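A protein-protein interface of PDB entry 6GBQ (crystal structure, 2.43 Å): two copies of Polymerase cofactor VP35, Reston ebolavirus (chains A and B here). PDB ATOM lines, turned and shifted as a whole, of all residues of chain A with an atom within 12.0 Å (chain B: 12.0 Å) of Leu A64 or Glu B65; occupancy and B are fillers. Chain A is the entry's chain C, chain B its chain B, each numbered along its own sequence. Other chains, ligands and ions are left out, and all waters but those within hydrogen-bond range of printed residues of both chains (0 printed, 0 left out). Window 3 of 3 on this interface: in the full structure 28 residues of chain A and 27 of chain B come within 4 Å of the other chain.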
ATOM      1  N   ALA A  55      30.078 -20.183  18.384  1.00  0.00           N
ATOM      2  CA  ALA A  55      28.680 -20.213  17.918  1.00  0.00           C
ATOM      3  C   ALA A  55      28.047 -18.819  17.960  1.00  0.00           C
ATOM      4  O   ALA A  55      27.290 -18.450  17.061  1.00  0.00           O
ATOM      5  CB  ALA A  55      27.863 -21.196  18.745  1.00  0.00           C
ATOM      6  N   GLU A  56      28.381 -18.048  18.994  1.00  0.00           N
ATOM      7  CA  GLU A  56      27.910 -16.663  19.139  1.00  0.00           C
ATOM      8  C   GLU A  56      28.480 -15.731  18.058  1.00  0.00           C
ATOM      9  O   GLU A  56      27.774 -14.851  17.574  1.00  0.00           O
ATOM     10  CB  GLU A  56      28.238 -16.122  20.542  1.00  0.00           C
ATOM     11  CG  GLU A  56      27.570 -14.793  20.860  1.00  0.00           C
ATOM     12  CD  GLU A  56      27.785 -14.304  22.286  1.00  0.00           C
ATOM     13  OE1 GLU A  56      28.431 -15.004  23.098  1.00  0.00           O
ATOM     14  OE2 GLU A  56      27.299 -13.188  22.594  1.00  0.00           O
ATOM     15  N   MET A  57      29.749 -15.921  17.695  1.00  0.00           N
ATOM     16  CA  MET A  57      30.372 -15.167  16.597  1.00  0.00           C
ATOM     17  C   MET A  57      29.748 -15.525  15.241  1.00  0.00           C
ATOM     18  O   MET A  57      29.499 -14.639  14.425  1.00  0.00           O
ATOM     19  CB  MET A  57      31.885 -15.434  16.555  1.00  0.00           C
ATOM     20  CG  MET A  57      32.652 -14.639  15.508  1.00  0.00           C
ATOM     21  SD  MET A  57      34.413 -15.025  15.495  1.00  0.00           S
ATOM     22  CE  MET A  57      34.424 -16.557  14.568  1.00  0.00           C
ATOM     23  N   VAL A  58      29.506 -16.816  15.012  1.00  0.00           N
ATOM     24  CA  VAL A  58      28.841 -17.282  13.793  1.00  0.00           C
ATOM     25  C   VAL A  58      27.481 -16.593  13.643  1.00  0.00           C
ATOM     26  O   VAL A  58      27.261 -15.884  12.666  1.00  0.00           O
ATOM     27  CB  VAL A  58      28.668 -18.826  13.772  1.00  0.00           C
ATOM     28  CG1 VAL A  58      27.771 -19.275  12.621  1.00  0.00           C
ATOM     29  CG2 VAL A  58      30.022 -19.527  13.669  1.00  0.00           C
ATOM     30  N   ALA A  59      26.601 -16.766  14.627  1.00  0.00           N
ATOM     31  CA  ALA A  59      25.253 -16.188  14.580  1.00  0.00           C
ATOM     32  C   ALA A  59      25.266 -14.705  14.261  1.00  0.00           C
ATOM     33  O   ALA A  59      24.492 -14.250  13.427  1.00  0.00           O
ATOM     34  CB  ALA A  59      24.513 -16.426  15.888  1.00  0.00           C
ATOM     35  N   LYS A  60      26.152 -13.957  14.912  1.00  0.00           N
ATOM     36  CA  LYS A  60      26.222 -12.504  14.722  1.00  0.00           C
ATOM     37  C   LYS A  60      26.831 -12.094  13.371  1.00  0.00           C
ATOM     38  O   LYS A  60      26.280 -11.228  12.689  1.00  0.00           O
ATOM     39  CB  LYS A  60      26.982 -11.839  15.873  1.00  0.00           C
ATOM     40  CG  LYS A  60      26.215 -11.799  17.190  1.00  0.00           C
ATOM     41  CD  LYS A  60      27.087 -11.206  18.295  1.00  0.00           C
ATOM     42  CE  LYS A  60      26.470 -11.321  19.687  1.00  0.00           C
ATOM     43  NZ  LYS A  60      25.383 -10.333  19.908  1.00  0.00           N
ATOM     44  N   TYR A  61      27.947 -12.715  12.985  1.00  0.00           N
ATOM     45  CA  TYR A  61      28.670 -12.341  11.747  1.00  0.00           C
ATOM     46  C   TYR A  61      28.052 -12.907  10.450  1.00  0.00           C
ATOM     47  O   TYR A  61      28.163 -12.281   9.398  1.00  0.00           O
ATOM     48  CB  TYR A  61      30.151 -12.744  11.826  1.00  0.00           C
ATOM     49  CG  TYR A  61      31.046 -11.794  12.614  1.00  0.00           C
ATOM     50  CD1 TYR A  61      31.153 -11.889  14.003  1.00  0.00           C
ATOM     51  CD2 TYR A  61      31.807 -10.815  11.967  1.00  0.00           C
ATOM     52  CE1 TYR A  61      31.965 -11.032  14.719  1.00  0.00           C
ATOM     53  CE2 TYR A  61      32.625  -9.954  12.680  1.00  0.00           C
ATOM     54  CZ  TYR A  61      32.701 -10.067  14.057  1.00  0.00           C
ATOM     55  OH  TYR A  61      33.517  -9.223  14.779  1.00  0.00           O
ATOM     56  N   ASP A  62      27.437 -14.091  10.525  1.00  0.00           N
ATOM     57  CA  ASP A  62      26.651 -14.660   9.410  1.00  0.00           C
ATOM     58  C   ASP A  62      25.529 -13.706   9.009  1.00  0.00           C
ATOM     59  O   ASP A  62      25.336 -13.429   7.822  1.00  0.00           O
ATOM     60  CB  ASP A  62      26.050 -16.020   9.808  1.00  0.00           C
ATOM     61  CG  ASP A  62      25.435 -16.781   8.626  1.00  0.00           C
ATOM     62  OD1 ASP A  62      24.608 -16.214   7.869  1.00  0.00           O
ATOM     63  OD2 ASP A  62      25.770 -17.977   8.473  1.00  0.00           O
ATOM     64  N   LEU A  63      24.791 -13.227  10.008  1.00  0.00           N
ATOM     65  CA  LEU A  63      23.757 -12.201   9.825  1.00  0.00           C
ATOM     66  C   LEU A  63      24.278 -11.001   9.021  1.00  0.00           C
ATOM     67  O   LEU A  63      23.600 -10.506   8.119  1.00  0.00           O
ATOM     68  CB  LEU A  63      23.240 -11.735  11.196  1.00  0.00           C
ATOM     69  CG  LEU A  63      22.089 -10.733  11.253  1.00  0.00           C
ATOM     70  CD1 LEU A  63      20.858 -11.304  10.568  1.00  0.00           C
ATOM     71  CD2 LEU A  63      21.783 -10.371  12.703  1.00  0.00           C
ATOM     72  N   LEU A  64      25.492 -10.565   9.345  1.00  0.00           N
ATOM     73  CA  LEU A  64      26.141  -9.433   8.678  1.00  0.00           C
ATOM     74  C   LEU A  64      26.595  -9.737   7.240  1.00  0.00           C
ATOM     75  O   LEU A  64      26.605  -8.842   6.397  1.00  0.00           O
ATOM     76  CB  LEU A  64      27.322  -8.945   9.528  1.00  0.00           C
ATOM     77  CG  LEU A  64      27.813  -7.520   9.263  1.00  0.00           C
ATOM     78  CD1 LEU A  64      28.103  -6.793  10.565  1.00  0.00           C
ATOM     79  CD2 LEU A  64      29.037  -7.510   8.361  1.00  0.00           C
ATOM     80  N   GLU A  65      26.984 -10.983   6.968  1.00  0.00           N
ATOM     81  CA  GLU A  65      27.283 -11.417   5.599  1.00  0.00           C
ATOM     82  C   GLU A  65      26.004 -11.552   4.778  1.00  0.00           C
ATOM     83  O   GLU A  65      26.033 -11.368   3.559  1.00  0.00           O
ATOM     84  CB  GLU A  65      28.047 -12.746   5.593  1.00  0.00           C
ATOM     85  N   HIS A  66      24.895 -11.881   5.445  1.00  0.00           N
ATOM     86  CA  HIS A  66      23.575 -11.967   4.806  1.00  0.00           C
ATOM     87  C   HIS A  66      23.084 -10.602   4.326  1.00  0.00           C
ATOM     88  O   HIS A  66      22.631 -10.474   3.187  1.00  0.00           O
ATOM     89  CB  HIS A  66      22.539 -12.583   5.761  1.00  0.00           C
ATOM     90  N   HIS A  67      23.184  -9.591   5.190  1.00  0.00           N
ATOM     91  CA  HIS A  67      22.744  -8.228   4.853  1.00  0.00           C
ATOM     92  C   HIS A  67      23.656  -7.526   3.850  1.00  0.00           C
ATOM     93  O   HIS A  67      23.171  -6.762   3.011  1.00  0.00           O
ATOM     94  CB  HIS A  67      22.584  -7.378   6.113  1.00  0.00           C
ATOM     95  CG  HIS A  67      21.492  -7.856   7.015  1.00  0.00           C
ATOM     96  ND1 HIS A  67      21.645  -7.963   8.382  1.00  0.00           N
ATOM     97  CD2 HIS A  67      20.235  -8.284   6.743  1.00  0.00           C
ATOM     98  CE1 HIS A  67      20.524  -8.419   8.913  1.00  0.00           C
ATOM     99  NE2 HIS A  67      19.654  -8.627   7.939  1.00  0.00           N
ATOM    100  N   HIS A  68      24.963  -7.777   3.939  1.00  0.00           N
ATOM    101  CA  HIS A  68      25.919  -7.289   2.937  1.00  0.00           C
ATOM    102  C   HIS A  68      25.667  -7.896   1.542  1.00  0.00           C
ATOM    103  O   HIS A  68      25.804  -7.199   0.539  1.00  0.00           O
ATOM    104  CB  HIS A  68      27.361  -7.557   3.390  1.00  0.00           C
ATOM    105  CG  HIS A  68      28.402  -6.948   2.502  1.00  0.00           C
ATOM    106  ND1 HIS A  68      29.034  -7.656   1.502  1.00  0.00           N
ATOM    107  CD2 HIS A  68      28.921  -5.697   2.462  1.00  0.00           C
ATOM    108  CE1 HIS A  68      29.897  -6.870   0.884  1.00  0.00           C
ATOM    109  NE2 HIS A  68      29.848  -5.675   1.445  1.00  0.00           N
ATOM    110  N   HIS A  69      25.280  -9.174   1.492  1.00  0.00           N
ATOM    111  CA  HIS A  69      25.048  -9.898   0.228  1.00  0.00           C
ATOM    112  C   HIS A  69      23.604  -9.868  -0.295  1.00  0.00           C
ATOM    113  O   HIS A  69      23.378 -10.185  -1.466  1.00  0.00           O
ATOM    114  CB  HIS A  69      25.479 -11.359   0.373  1.00  0.00           C
ATOM    115  N   HIS A  70      22.636  -9.523   0.560  1.00  0.00           N
ATOM    116  CA  HIS A  70      21.221  -9.444   0.161  1.00  0.00           C
ATOM    117  C   HIS A  70      20.429  -8.504   1.065  1.00  0.00           C
ATOM    118  O   HIS A  70      20.060  -7.401   0.660  1.00  0.00           O
ATOM    119  CB  HIS A  70      20.579 -10.834   0.185  1.00  0.00           C
ATOM    120  N   GLU B  56      36.739 -11.908  21.435  1.00  0.00           N
ATOM    121  CA  GLU B  56      37.135 -10.565  20.971  1.00  0.00           C
ATOM    122  C   GLU B  56      36.325 -10.083  19.769  1.00  0.00           C
ATOM    123  O   GLU B  56      35.949  -8.923  19.700  1.00  0.00           O
ATOM    124  CB  GLU B  56      38.633 -10.526  20.648  1.00  0.00           C
ATOM    125  CG  GLU B  56      39.493 -10.516  21.904  1.00  0.00           C
ATOM    126  CD  GLU B  56      40.935 -10.972  21.707  1.00  0.00           C
ATOM    127  OE1 GLU B  56      41.281 -11.547  20.654  1.00  0.00           O
ATOM    128  OE2 GLU B  56      41.733 -10.762  22.638  1.00  0.00           O
ATOM    129  N   MET B  57      36.065 -10.982  18.831  1.00  0.00           N
ATOM    130  CA  MET B  57      35.212 -10.688  17.681  1.00  0.00           C
ATOM    131  C   MET B  57      33.763 -10.396  18.075  1.00  0.00           C
ATOM    132  O   MET B  57      33.128  -9.507  17.491  1.00  0.00           O
ATOM    133  CB  MET B  57      35.254 -11.850  16.690  1.00  0.00           C
ATOM    134  CG  MET B  57      36.599 -12.011  15.993  1.00  0.00           C
ATOM    135  SD  MET B  57      37.052 -10.556  15.028  1.00  0.00           S
ATOM    136  CE  MET B  57      35.996 -10.731  13.585  1.00  0.00           C
ATOM    137  N   VAL B  58      33.252 -11.126  19.067  1.00  0.00           N
ATOM    138  CA  VAL B  58      31.918 -10.870  19.597  1.00  0.00           C
ATOM    139  C   VAL B  58      31.870  -9.479  20.227  1.00  0.00           C
ATOM    140  O   VAL B  58      30.974  -8.690  19.917  1.00  0.00           O
ATOM    141  CB  VAL B  58      31.480 -11.948  20.619  1.00  0.00           C
ATOM    142  CG1 VAL B  58      30.197 -11.531  21.345  1.00  0.00           C
ATOM    143  CG2 VAL B  58      31.290 -13.294  19.917  1.00  0.00           C
ATOM    144  N   ALA B  59      32.840  -9.193  21.093  1.00  0.00           N
ATOM    145  CA  ALA B  59      32.975  -7.886  21.725  1.00  0.00           C
ATOM    146  C   ALA B  59      33.106  -6.751  20.710  1.00  0.00           C
ATOM    147  O   ALA B  59      32.491  -5.696  20.878  1.00  0.00           O
ATOM    148  CB  ALA B  59      34.154  -7.878  22.676  1.00  0.00           C
ATOM    149  N   LYS B  60      33.877  -6.978  19.648  1.00  0.00           N
ATOM    150  CA  LYS B  60      34.059  -5.962  18.598  1.00  0.00           C
ATOM    151  C   LYS B  60      32.781  -5.687  17.820  1.00  0.00           C
ATOM    152  O   LYS B  60      32.451  -4.538  17.554  1.00  0.00           O
ATOM    153  CB  LYS B  60      35.157  -6.379  17.627  1.00  0.00           C
ATOM    154  CG  LYS B  60      35.540  -5.282  16.648  1.00  0.00           C
ATOM    155  CD  LYS B  60      36.869  -5.581  15.991  1.00  0.00           C
ATOM    156  CE  LYS B  60      37.223  -4.504  14.977  1.00  0.00           C
ATOM    157  NZ  LYS B  60      38.419  -4.893  14.185  1.00  0.00           N
ATOM    158  N   TYR B  61      32.097  -6.757  17.437  1.00  0.00           N
ATOM    159  CA  TYR B  61      30.766  -6.680  16.835  1.00  0.00           C
ATOM    160  C   TYR B  61      29.806  -5.845  17.691  1.00  0.00           C
ATOM    161  O   TYR B  61      29.250  -4.864  17.210  1.00  0.00           O
ATOM    162  CB  TYR B  61      30.222  -8.097  16.633  1.00  0.00           C
ATOM    163  CG  TYR B  61      28.912  -8.186  15.888  1.00  0.00           C
ATOM    164  CD1 TYR B  61      27.701  -7.949  16.541  1.00  0.00           C
ATOM    165  CD2 TYR B  61      28.873  -8.538  14.543  1.00  0.00           C
ATOM    166  CE1 TYR B  61      26.492  -8.035  15.873  1.00  0.00           C
ATOM    167  CE2 TYR B  61      27.662  -8.629  13.868  1.00  0.00           C
ATOM    168  CZ  TYR B  61      26.477  -8.377  14.541  1.00  0.00           C
ATOM    169  OH  TYR B  61      25.272  -8.450  13.903  1.00  0.00           O
ATOM    170  N   ASP B  62      29.642  -6.236  18.959  1.00  0.00           N
ATOM    171  CA  ASP B  62      28.709  -5.569  19.889  1.00  0.00           C
ATOM    172  C   ASP B  62      29.041  -4.083  20.085  1.00  0.00           C
ATOM    173  O   ASP B  62      28.144  -3.239  20.191  1.00  0.00           O
ATOM    174  CB  ASP B  62      28.705  -6.270  21.256  1.00  0.00           C
ATOM    175  CG  ASP B  62      28.077  -7.664  21.220  1.00  0.00           C
ATOM    176  OD1 ASP B  62      27.340  -7.996  20.269  1.00  0.00           O
ATOM    177  OD2 ASP B  62      28.312  -8.433  22.172  1.00  0.00           O
ATOM    178  N   LEU B  63      30.332  -3.774  20.120  1.00  0.00           N
ATOM    179  CA  LEU B  63      30.793  -2.400  20.254  1.00  0.00           C
ATOM    180  C   LEU B  63      30.448  -1.542  19.025  1.00  0.00           C
ATOM    181  O   LEU B  63      29.719  -0.551  19.133  1.00  0.00           O
ATOM    182  CB  LEU B  63      32.306  -2.391  20.498  1.00  0.00           C
ATOM    183  CG  LEU B  63      32.969  -1.067  20.837  1.00  0.00           C
ATOM    184  CD1 LEU B  63      32.431  -0.523  22.146  1.00  0.00           C
ATOM    185  CD2 LEU B  63      34.471  -1.266  20.915  1.00  0.00           C
ATOM    186  N   LEU B  64      30.949  -1.939  17.859  1.00  0.00           N
ATOM    187  CA  LEU B  64      30.817  -1.124  16.645  1.00  0.00           C
ATOM    188  C   LEU B  64      29.387  -0.978  16.117  1.00  0.00           C
ATOM    189  O   LEU B  64      29.143  -0.109  15.280  1.00  0.00           O
ATOM    190  CB  LEU B  64      31.730  -1.652  15.526  1.00  0.00           C
ATOM    191  CG  LEU B  64      33.242  -1.480  15.717  1.00  0.00           C
ATOM    192  CD1 LEU B  64      33.986  -1.961  14.479  1.00  0.00           C
ATOM    193  CD2 LEU B  64      33.617  -0.040  16.022  1.00  0.00           C
ATOM    194  N   GLU B  65      28.458  -1.812  16.590  1.00  0.00           N
ATOM    195  CA  GLU B  65      27.076  -1.774  16.121  1.00  0.00           C
ATOM    196  C   GLU B  65      26.077  -1.431  17.222  1.00  0.00           C
ATOM    197  O   GLU B  65      25.512  -0.336  17.218  1.00  0.00           O
ATOM    198  CB  GLU B  65      26.741  -3.097  15.444  1.00  0.00           C
ATOM    199  CG  GLU B  65      27.773  -3.467  14.392  1.00  0.00           C
ATOM    200  CD  GLU B  65      27.196  -4.294  13.271  1.00  0.00           C
ATOM    201  OE1 GLU B  65      27.039  -5.524  13.440  1.00  0.00           O
ATOM    202  OE2 GLU B  65      26.907  -3.699  12.212  1.00  0.00           O
ATOM    203  N   HIS B  66      25.878  -2.341  18.172  1.00  0.00           N
ATOM    204  CA  HIS B  66      24.848  -2.182  19.203  1.00  0.00           C
ATOM    205  C   HIS B  66      25.379  -1.370  20.378  1.00  0.00           C
ATOM    206  O   HIS B  66      25.979  -0.310  20.189  1.00  0.00           O
ATOM    207  CB  HIS B  66      24.345  -3.551  19.675  1.00  0.00           C
ATOM    208  CG  HIS B  66      23.770  -4.390  18.574  1.00  0.00           C
ATOM    209  ND1 HIS B  66      23.863  -5.766  18.555  1.00  0.00           N
ATOM    210  CD2 HIS B  66      23.114  -4.043  17.440  1.00  0.00           C
ATOM    211  CE1 HIS B  66      23.272  -6.230  17.467  1.00  0.00           C
ATOM    212  NE2 HIS B  66      22.813  -5.204  16.772  1.00  0.00           N
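Ala A55 touches none of the printed residues of chain B.
Printed residues of chain B within 4 Å of Glu A56: Val B58 (3.6 Å).
Of the printed residues of chain B, Met A57 touches Met B57 (3.5 Å) and Val B58 (3.8 Å).
Tyr A61 touches just these residues of chain B: Met B57 and Tyr B61.
Leu A64 touches just these residues of chain B: Tyr B61 and Glu B65.
No residue of chain B comes within 4 Å of Glu A65.
No residue of chain B comes within 4 Å of His A66.
No residue of chain B comes within 4 Å of His A67.
His A68 touches none of the printed residues of chain B.
Of the printed residues of chain A, Met B57 touches Met A57 (3.5 Å) and Tyr A61 (2.8 Å).
Printed residues of chain A within 4 Å of Val B58: Glu A56 and Met A57.
Of the printed residues of chain A, Tyr B61 touches Lys A60, Tyr A61 and Leu A64.
Of the printed residues of chain A, Glu B65 touches Leu A64 (3.3 Å).
The nearest residue of chain B that does not touch Leu A64 is Leu B64 (8.0 Å).
The nearest printed residue of chain A that does not touch Asp B62 is Glu A56 (4.9 Å).
Glu A56 touches Val B58, but with the chains exchanged Val A58 does not touch Glu B56 (10.7 Å).
Met A57 touches Val B58, but with the chains exchanged Val A58 does not touch Met B57 (7.8 Å).
Lys A60 touches Tyr B61, but with the chains exchanged Tyr A61 does not touch Lys B60 (4.3 Å).
Tyr A61 touches its own counterpart, Tyr B61.
Of the 9 pairs that touch across the chains among the printed residues, 2 have their exchanged pair printed and touching as well.
OE1 of Glu B65 lies close to OH of Tyr B61, at 3.4 Å.
Of the 16 printed residues of chain A, 5 touch a printed residue of chain B.
Among the printed residues, 9 pairs touch across the chains.
Among the printed residues, Asp or Glu carboxylates within 4 Å of a Lys or Arg side-chain nitrogen of the other chain: Lys A60 with Asp B62 (3.1 Å).
Among the printed residues, merely in contact across the chains: Glu A56 with Val B58, Met A57 with Met B57, Met A57 with Val B58, Tyr A61 with Tyr B61, Leu A64 with Tyr B61 and Leu A64 with Glu B65.
The backbone carbonyl oxygen (O) of Met B57 lies within hydrogen-bond range of the side-chain hydroxyl (OH) of Tyr A61, at 2.8 Å.
O of Lys A60 lies close to OH of Tyr B61 (3.2 Å).
NZ of Lys A60 is in salt-bridge range of OD1 of Asp B62 (3.1 Å).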
